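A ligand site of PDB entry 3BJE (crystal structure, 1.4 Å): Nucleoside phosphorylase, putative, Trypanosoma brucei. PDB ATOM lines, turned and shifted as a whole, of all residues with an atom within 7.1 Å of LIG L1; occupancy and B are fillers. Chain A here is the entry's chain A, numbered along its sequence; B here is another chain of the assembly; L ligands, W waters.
A ring nitrogen (NE2) of His 34 of chain B is in hydrogen-bond range of an oxygen (O1) of LG2 L2, at 2.8 Å.
O7 of LG2 L2 is in salt-bridge range of NH2 of Arg 145.
An oxygen (O4) of LG2 L2 sits at hydrogen-bond distance from the side-chain carboxylate of Glu 294 (2.5 Å).
The backbone NH of Met 293 is in hydrogen-bond range of an oxygen (O3) of LG2 L2, 3.0 Å away.
The guanidinium group (NH2) of Arg 256 lies within hydrogen-bond range of an oxygen (O2) of LIG L1 (2.9 Å).
A nitrogen (N2) of LIG L1 sits at hydrogen-bond distance from the side-chain amide oxygen of Gln 254, 2.8 Å away.
OG1 of Thr 148 lies within hydrogen-bond range of O8 of LG2 L2, 2.8 Å away.
NH1 of Arg 74 of chain B is in salt-bridge range of O6 of LG2 L2 (2.9 Å).
O of Thr 148 touches N1 of LIG L1, 3.9 Å away.
C of Cys 149 touches C3 of LIG L1 (3.3 Å).
Gly 150 touches LIG L1 (N to C2, 3.3 Å).
Phe 250 touches LIG L1 (CE1 to N2, 3.5 Å).
O of Ile 291 touches N2 of LIG L1 (3.7 Å).
CA of Glu 292 touches O1 of LIG L1, at 3.4 Å.
CG of Met 293 touches O1 of LIG L1, 3.6 Å away.
Val 316 touches LIG L1.
CB of Ser 317 touches O2 of LIG L1 (3.7 Å).
Hydrophobic or aromatic side chains within 4 Å of LIG L1: Phe 250, Met 293 and Val 316.
The nearest printed residue that does not touch LIG L1 is Arg 319 (4.4 Å).
The backbone NH (N) of Cys 149 is in hydrogen-bond range of the backbone carbonyl oxygen (O) of Val 314, at 2.9 Å.
The side-chain carboxylate (OE1) of Glu 292 lies within salt-bridge range of the guanidinium group (NE) of Arg 145, 3.0 Å away.
The guanidinium group (NH1) of Arg 145 is in hydrogen-bond range of the backbone carbonyl oxygen (O) of Thr 148, at 3.3 Å.
NH1 of Arg 256 is in hydrogen-bond range of O of Phe 250 (2.9 Å).
The side-chain amide oxygen (OE1) of Gln 254 sits at hydrogen-bond distance from the guanidinium group (NH1) of Arg 256 (3.2 Å).
The backbone NH (N) of Val 316 lies within hydrogen-bond range of the backbone carbonyl oxygen (O) of Cys 149, at 2.9 Å.
O of Cys 149 sits at hydrogen-bond distance from N of Ser 317, at 3.4 Å.
OE1 of Glu 292 is in hydrogen-bond range of N of Glu 294, at 3.0 Å.
Water W2 lies within hydrogen-bond range of O2 of LIG L1 (2.7 Å), OE1 of Gln 254 (2.8 Å) and NH1 of Arg 319 (2.9 Å).
Water W1 lies within hydrogen-bond range of an oxygen (O1) of LG2 L2 (2.7 Å) and the side-chain hydroxyl (OG1) of Thr 148 (3.1 Å).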
ATOM      1  N   ARG A 145      23.702  -7.180   9.819  1.00  0.00           N
ATOM      2  CA  ARG A 145      23.920  -8.491   9.211  1.00  0.00           C
ATOM      3  C   ARG A 145      23.630  -8.414   7.730  1.00  0.00           C
ATOM      4  O   ARG A 145      22.595  -7.900   7.337  1.00  0.00           O
ATOM      5  CB  ARG A 145      23.015  -9.527   9.877  1.00  0.00           C
ATOM      6  CG  ARG A 145      22.880 -10.815   9.076  1.00  0.00           C
ATOM      7  CD  ARG A 145      22.279 -11.924   9.916  1.00  0.00           C
ATOM      8  NE  ARG A 145      21.707 -12.986   9.075  1.00  0.00           N
ATOM      9  CZ  ARG A 145      22.413 -13.791   8.282  1.00  0.00           C
ATOM     10  NH1 ARG A 145      21.774 -14.693   7.557  1.00  0.00           N
ATOM     11  NH2 ARG A 145      23.745 -13.710   8.193  1.00  0.00           N
ATOM     12  N   THR A 148      22.306 -14.571   3.840  1.00  0.00           N
ATOM     13  CA  THR A 148      21.469 -15.248   2.866  1.00  0.00           C
ATOM     14  C   THR A 148      20.280 -15.807   3.618  1.00  0.00           C
ATOM     15  O   THR A 148      20.313 -15.947   4.822  1.00  0.00           O
ATOM     16  CB  THR A 148      22.215 -16.393   2.144  1.00  0.00           C
ATOM     17  OG1 THR A 148      22.647 -17.390   3.084  1.00  0.00           O
ATOM     18  CG2 THR A 148      23.406 -15.831   1.322  1.00  0.00           C
ATOM     19  N   CYS A 149      19.206 -16.103   2.899  1.00  0.00           N
ATOM     20  CA  CYS A 149      18.005 -16.586   3.585  1.00  0.00           C
ATOM     21  C   CYS A 149      17.062 -17.312   2.663  1.00  0.00           C
ATOM     22  O   CYS A 149      17.253 -17.354   1.441  1.00  0.00           O
ATOM     23  CB  CYS A 149      17.272 -15.388   4.206  1.00  0.00           C
ATOM     24  SG  CYS A 149      16.576 -14.264   2.931  1.00  0.00           S
ATOM     25  N   GLY A 150      16.034 -17.914   3.266  1.00  0.00           N
ATOM     26  CA  GLY A 150      14.888 -18.411   2.507  1.00  0.00           C
ATOM     27  C   GLY A 150      13.736 -17.431   2.608  1.00  0.00           C
ATOM     28  O   GLY A 150      13.734 -16.580   3.508  1.00  0.00           O
ATOM     29  N   SER A 151      12.798 -17.526   1.662  1.00  0.00           N
ATOM     30  CA  SER A 151      11.552 -16.754   1.769  1.00  0.00           C
ATOM     31  C   SER A 151      10.332 -17.648   1.593  1.00  0.00           C
ATOM     32  O   SER A 151      10.262 -18.407   0.627  1.00  0.00           O
ATOM     33  CB  SER A 151      11.479 -15.618   0.751  1.00  0.00           C
ATOM     34  OG  SER A 151      10.219 -14.961   0.821  1.00  0.00           O
ATOM     35  N   ALA A 247      15.528 -19.365  12.950  1.00  0.00           N
ATOM     36  CA  ALA A 247      15.445 -20.765  13.303  1.00  0.00           C
ATOM     37  C   ALA A 247      16.694 -21.249  14.024  1.00  0.00           C
ATOM     38  O   ALA A 247      17.789 -20.675  13.857  1.00  0.00           O
ATOM     39  CB  ALA A 247      15.289 -21.605  12.024  1.00  0.00           C
ATOM     40  N   GLY A 249      18.094 -24.132  13.472  1.00  0.00           N
ATOM     41  CA  GLY A 249      18.576 -25.161  12.542  1.00  0.00           C
ATOM     42  C   GLY A 249      18.201 -24.770  11.134  1.00  0.00           C
ATOM     43  O   GLY A 249      17.680 -23.679  10.909  1.00  0.00           O
ATOM     44  N   PHE A 250      18.490 -25.653  10.186  1.00  0.00           N
ATOM     45  CA  PHE A 250      18.257 -25.405   8.773  1.00  0.00           C
ATOM     46  C   PHE A 250      17.154 -26.281   8.152  1.00  0.00           C
ATOM     47  O   PHE A 250      16.518 -25.895   7.180  1.00  0.00           O
ATOM     48  CB  PHE A 250      19.552 -25.654   8.019  1.00  0.00           C
ATOM     49  CG  PHE A 250      19.500 -25.267   6.572  1.00  0.00           C
ATOM     50  CD1 PHE A 250      19.788 -23.963   6.207  1.00  0.00           C
ATOM     51  CD2 PHE A 250      19.204 -26.177   5.584  1.00  0.00           C
ATOM     52  CE1 PHE A 250      19.773 -23.577   4.880  1.00  0.00           C
ATOM     53  CE2 PHE A 250      19.204 -25.807   4.256  1.00  0.00           C
ATOM     54  CZ  PHE A 250      19.480 -24.508   3.897  1.00  0.00           C
ATOM     55  N   GLN A 254      13.448 -25.462  10.025  1.00  0.00           N
ATOM     56  CA  GLN A 254      12.837 -24.552   9.055  1.00  0.00           C
ATOM     57  C   GLN A 254      11.701 -25.231   8.248  1.00  0.00           C
ATOM     58  O   GLN A 254      11.320 -24.752   7.213  1.00  0.00           O
ATOM     59  CB  GLN A 254      13.885 -23.930   8.129  1.00  0.00           C
ATOM     60  CG  GLN A 254      14.963 -23.151   8.872  1.00  0.00           C
ATOM     61  CD  GLN A 254      15.946 -22.392   7.988  1.00  0.00           C
ATOM     62  OE1 GLN A 254      15.624 -22.054   6.824  1.00  0.00           O
ATOM     63  NE2 GLN A 254      17.121 -22.083   8.543  1.00  0.00           N
ATOM     64  N   ARG A 256      11.800 -28.105   6.636  1.00  0.00           N
ATOM     65  CA  ARG A 256      12.248 -29.012   5.580  1.00  0.00           C
ATOM     66  C   ARG A 256      12.021 -30.455   5.998  1.00  0.00           C
ATOM     67  O   ARG A 256      12.278 -30.829   7.145  1.00  0.00           O
ATOM     68  CB  ARG A 256      13.729 -28.783   5.229  1.00  0.00           C
ATOM     69  CG  ARG A 256      14.016 -27.455   4.536  1.00  0.00           C
ATOM     70  CD  ARG A 256      15.475 -27.295   4.171  1.00  0.00           C
ATOM     71  NE  ARG A 256      15.640 -26.223   3.205  1.00  0.00           N
ATOM     72  CZ  ARG A 256      15.785 -24.931   3.487  1.00  0.00           C
ATOM     73  NH1 ARG A 256      15.861 -24.502   4.729  1.00  0.00           N
ATOM     74  NH2 ARG A 256      15.876 -24.051   2.502  1.00  0.00           N
ATOM     75  N   ILE A 291      13.297 -16.288   6.183  1.00  0.00           N
ATOM     76  CA  ILE A 291      13.671 -17.223   7.254  1.00  0.00           C
ATOM     77  C   ILE A 291      15.175 -17.444   7.175  1.00  0.00           C
ATOM     78  O   ILE A 291      15.705 -17.713   6.082  1.00  0.00           O
ATOM     79  CB  ILE A 291      12.984 -18.601   7.079  1.00  0.00           C
ATOM     80  CG1 ILE A 291      11.471 -18.459   7.051  1.00  0.00           C
ATOM     81  CG2 ILE A 291      13.453 -19.597   8.174  1.00  0.00           C
ATOM     82  CD1 ILE A 291      10.733 -19.686   6.474  1.00  0.00           C
ATOM     83  N   GLU A 292      15.851 -17.363   8.309  1.00  0.00           N
ATOM     84  CA  GLU A 292      17.300 -17.582   8.378  1.00  0.00           C
ATOM     85  C   GLU A 292      17.679 -17.967   9.828  1.00  0.00           C
ATOM     86  O   GLU A 292      16.805 -18.408  10.607  1.00  0.00           O
ATOM     87  CB  GLU A 292      18.088 -16.389   7.816  1.00  0.00           C
ATOM     88  CG  GLU A 292      17.644 -14.998   8.315  1.00  0.00           C
ATOM     89  CD  GLU A 292      18.007 -14.792   9.764  1.00  0.00           C
ATOM     90  OE1 GLU A 292      19.166 -14.371  10.006  1.00  0.00           O
ATOM     91  OE2 GLU A 292      17.144 -15.077  10.624  1.00  0.00           O
ATOM     92  N   MET A 293      18.954 -17.824  10.200  1.00  0.00           N
ATOM     93  CA  MET A 293      19.425 -18.420  11.461  1.00  0.00           C
ATOM     94  C   MET A 293      20.080 -17.488  12.489  1.00  0.00           C
ATOM     95  O   MET A 293      20.549 -17.971  13.521  1.00  0.00           O
ATOM     96  CB  MET A 293      20.377 -19.587  11.144  1.00  0.00           C
ATOM     97  CG  MET A 293      19.696 -20.720  10.409  1.00  0.00           C
ATOM     98  SD  MET A 293      20.759 -22.105   9.976  1.00  0.00           S
ATOM     99  CE  MET A 293      21.238 -22.706  11.635  1.00  0.00           C
ATOM    100  N   GLU A 294      20.107 -16.172  12.246  1.00  0.00           N
ATOM    101  CA  GLU A 294      20.807 -15.229  13.149  1.00  0.00           C
ATOM    102  C   GLU A 294      20.058 -13.989  13.626  1.00  0.00           C
ATOM    103  O   GLU A 294      20.384 -13.434  14.671  1.00  0.00           O
ATOM    104  CB  GLU A 294      22.116 -14.768  12.479  1.00  0.00           C
ATOM    105  CG  GLU A 294      23.163 -15.887  12.333  1.00  0.00           C
ATOM    106  CD  GLU A 294      23.142 -16.586  10.972  1.00  0.00           C
ATOM    107  OE1 GLU A 294      22.816 -15.956   9.955  1.00  0.00           O
ATOM    108  OE2 GLU A 294      23.459 -17.811  10.897  1.00  0.00           O
ATOM    109  N   VAL A 314      20.067 -11.826   1.275  1.00  0.00           N
ATOM    110  CA  VAL A 314      19.756 -12.188  -0.089  1.00  0.00           C
ATOM    111  C   VAL A 314      18.938 -13.490  -0.095  1.00  0.00           C
ATOM    112  O   VAL A 314      19.330 -14.475   0.518  1.00  0.00           O
ATOM    113  CB  VAL A 314      21.061 -12.345  -0.934  1.00  0.00           C
ATOM    114  CG1 VAL A 314      20.767 -12.770  -2.377  1.00  0.00           C
ATOM    115  CG2 VAL A 314      21.874 -11.047  -0.937  1.00  0.00           C
ATOM    116  N   VAL A 315      17.830 -13.487  -0.849  1.00  0.00           N
ATOM    117  CA  VAL A 315      16.941 -14.654  -0.900  1.00  0.00           C
ATOM    118  C   VAL A 315      17.553 -15.689  -1.839  1.00  0.00           C
ATOM    119  O   VAL A 315      17.533 -15.511  -3.050  1.00  0.00           O
ATOM    120  CB  VAL A 315      15.515 -14.273  -1.328  1.00  0.00           C
ATOM    121  CG1 VAL A 315      14.583 -15.510  -1.463  1.00  0.00           C
ATOM    122  CG2 VAL A 315      14.918 -13.290  -0.345  1.00  0.00           C
ATOM    123  N   VAL A 316      18.120 -16.756  -1.277  1.00  0.00           N
ATOM    124  CA  VAL A 316      18.749 -17.815  -2.056  1.00  0.00           C
ATOM    125  C   VAL A 316      17.914 -19.101  -2.139  1.00  0.00           C
ATOM    126  O   VAL A 316      18.257 -20.016  -2.872  1.00  0.00           O
ATOM    127  CB  VAL A 316      20.152 -18.166  -1.525  1.00  0.00           C
ATOM    128  CG1 VAL A 316      21.055 -16.935  -1.546  1.00  0.00           C
ATOM    129  CG2 VAL A 316      20.056 -18.752  -0.108  1.00  0.00           C
ATOM    130  N   SER A 317      16.822 -19.147  -1.391  1.00  0.00           N
ATOM    131  CA  SER A 317      15.931 -20.299  -1.435  1.00  0.00           C
ATOM    132  C   SER A 317      14.500 -19.808  -1.441  1.00  0.00           C
ATOM    133  O   SER A 317      14.064 -19.079  -0.549  1.00  0.00           O
ATOM    134  CB  SER A 317      16.149 -21.198  -0.227  1.00  0.00           C
ATOM    135  OG  SER A 317      15.200 -22.254  -0.219  1.00  0.00           O
ATOM    136  N   LYS A 318      13.771 -20.172  -2.483  1.00  0.00           N
ATOM    137  CA  LYS A 318      12.354 -19.880  -2.545  1.00  0.00           C
ATOM    138  C   LYS A 318      11.697 -21.183  -2.176  1.00  0.00           C
ATOM    139  O   LYS A 318      11.844 -22.187  -2.874  1.00  0.00           O
ATOM    140  CB  LYS A 318      11.910 -19.402  -3.928  1.00  0.00           C
ATOM    141  CG  LYS A 318      12.137 -17.912  -4.190  1.00  0.00           C
ATOM    142  CD  LYS A 318      11.381 -16.972  -3.225  1.00  0.00           C
ATOM    143  CE  LYS A 318       9.855 -17.101  -3.263  1.00  0.00           C
ATOM    144  NZ  LYS A 318       9.226 -16.367  -4.385  1.00  0.00           N
ATOM    145  N   ARG A 319      11.011 -21.151  -1.052  1.00  0.00           N
ATOM    146  CA  ARG A 319      10.419 -22.320  -0.469  1.00  0.00           C
ATOM    147  C   ARG A 319       8.990 -22.487  -1.016  1.00  0.00           C
ATOM    148  O   ARG A 319       8.381 -23.535  -0.830  1.00  0.00           O
ATOM    149  CB  ARG A 319      10.440 -22.163   1.066  1.00  0.00           C
ATOM    150  CG  ARG A 319      11.868 -21.911   1.677  1.00  0.00           C
ATOM    151  CD  ARG A 319      12.714 -23.189   1.784  1.00  0.00           C
ATOM    152  NE  ARG A 319      11.988 -24.331   2.371  1.00  0.00           N
ATOM    153  CZ  ARG A 319      11.840 -24.554   3.682  1.00  0.00           C
ATOM    154  NH1 ARG A 319      12.375 -23.737   4.584  1.00  0.00           N
ATOM    155  NH2 ARG A 319      11.148 -25.616   4.091  1.00  0.00           N
ATOM    156  N   MET A 325      16.646 -23.234  -5.374  1.00  0.00           N
ATOM    157  CA  MET A 325      17.729 -22.457  -4.758  1.00  0.00           C
ATOM    158  C   MET A 325      18.502 -21.687  -5.826  1.00  0.00           C
ATOM    159  O   MET A 325      18.606 -22.133  -6.970  1.00  0.00           O
ATOM    160  CB  MET A 325      18.682 -23.352  -3.977  1.00  0.00           C
ATOM    161  CG  MET A 325      18.116 -23.803  -2.624  1.00  0.00           C
ATOM    162  SD  MET A 325      19.454 -24.284  -1.510  1.00  0.00           S
ATOM    163  CE  MET A 325      20.151 -22.693  -1.077  1.00  0.00           C
ATOM    164  N   LEU B  33      24.796 -29.501   1.134  1.00  0.00           N
ATOM    165  CA  LEU B  33      24.908 -28.061   1.042  1.00  0.00           C
ATOM    166  C   LEU B  33      26.021 -27.438   1.888  1.00  0.00           C
ATOM    167  O   LEU B  33      26.653 -26.457   1.463  1.00  0.00           O
ATOM    168  CB  LEU B  33      23.568 -27.441   1.410  1.00  0.00           C
ATOM    169  CG  LEU B  33      23.337 -25.958   1.204  1.00  0.00           C
ATOM    170  CD1 LEU B  33      23.590 -25.559  -0.256  1.00  0.00           C
ATOM    171  CD2 LEU B  33      21.922 -25.604   1.612  1.00  0.00           C
ATOM    172  N   HIS B  34      26.229 -27.968   3.084  1.00  0.00           N
ATOM    173  CA  HIS B  34      27.203 -27.431   4.031  1.00  0.00           C
ATOM    174  C   HIS B  34      28.406 -28.361   4.176  1.00  0.00           C
ATOM    175  O   HIS B  34      29.556 -27.951   4.004  1.00  0.00           O
ATOM    176  CB  HIS B  34      26.541 -27.171   5.402  1.00  0.00           C
ATOM    177  CG  HIS B  34      25.374 -26.225   5.315  1.00  0.00           C
ATOM    178  ND1 HIS B  34      24.106 -26.634   4.958  1.00  0.00           N
ATOM    179  CD2 HIS B  34      25.297 -24.888   5.510  1.00  0.00           C
ATOM    180  CE1 HIS B  34      23.294 -25.594   4.947  1.00  0.00           C
ATOM    181  NE2 HIS B  34      23.995 -24.520   5.282  1.00  0.00           N
ATOM    182  N   ARG B  74      32.778 -23.184   4.712  1.00  0.00           N
ATOM    183  CA  ARG B  74      32.334 -22.505   5.943  1.00  0.00           C
ATOM    184  C   ARG B  74      33.130 -23.115   7.145  1.00  0.00           C
ATOM    185  O   ARG B  74      34.303 -23.398   7.026  1.00  0.00           O
ATOM    186  CB  ARG B  74      30.815 -22.657   6.138  1.00  0.00           C
ATOM    187  CG  ARG B  74      29.958 -21.909   5.135  1.00  0.00           C
ATOM    188  CD  ARG B  74      28.484 -22.294   5.317  1.00  0.00           C
ATOM    189  NE  ARG B  74      27.564 -21.516   4.469  1.00  0.00           N
ATOM    190  CZ  ARG B  74      27.049 -20.329   4.792  1.00  0.00           C
ATOM    191  NH1 ARG B  74      27.378 -19.756   5.932  1.00  0.00           N
ATOM    192  NH2 ARG B  74      26.197 -19.722   3.957  1.00  0.00           N
HETATM  193  N1  LIG L   1      19.610 -19.734   4.851  1.00  0.00           N
HETATM  194  C1  LIG L   1      18.687 -20.259   5.690  1.00  0.00           C
HETATM  195  O1  LIG L   1      18.866 -20.255   6.955  1.00  0.00           O
HETATM  196  N2  LIG L   1      17.588 -20.817   5.204  1.00  0.00           N
HETATM  197  C2  LIG L   1      17.367 -20.874   3.872  1.00  0.00           C
HETATM  198  O2  LIG L   1      16.311 -21.401   3.483  1.00  0.00           O
HETATM  199  C3  LIG L   1      18.299 -20.356   2.997  1.00  0.00           C
HETATM  200  C4  LIG L   1      19.438 -19.782   3.518  1.00  0.00           C
HETATM  201  C1  LG2 L   2      22.774 -21.426   6.497  1.00  0.00           C
HETATM  202  O1  LG2 L   2      23.105 -21.907   5.184  1.00  0.00           O
HETATM  203  C2  LG2 L   2      23.417 -20.086   6.761  1.00  0.00           C
HETATM  204  O2  LG2 L   2      23.156 -19.156   5.698  1.00  0.00           O
HETATM  205  C3  LG2 L   2      22.480 -17.996   6.191  1.00  0.00           C
HETATM  206  C4  LG2 L   2      21.818 -18.496   7.477  1.00  0.00           C
HETATM  207  O3  LG2 L   2      21.349 -17.492   8.409  1.00  0.00           O
HETATM  208  C5  LG2 L   2      22.893 -19.438   8.025  1.00  0.00           C
HETATM  209  O4  LG2 L   2      23.968 -18.726   8.666  1.00  0.00           O
HETATM  210  O5  LG2 L   2      23.360 -16.831   6.361  1.00  0.00           O
HETATM  211  P1  LG2 L   2      24.896 -16.646   5.920  1.00  0.00           P
HETATM  212  O6  LG2 L   2      25.564 -17.693   6.818  1.00  0.00           O
HETATM  213  O7  LG2 L   2      25.218 -15.214   6.296  1.00  0.00           O
HETATM  214  O8  LG2 L   2      25.053 -16.975   4.464  1.00  0.00           O
HETATM  215  O   HOH W   1      22.807 -20.455   2.909  1.00  0.00           O
HETATM  216  O   HOH W   2      13.900 -21.316   4.702  1.00  0.00           O
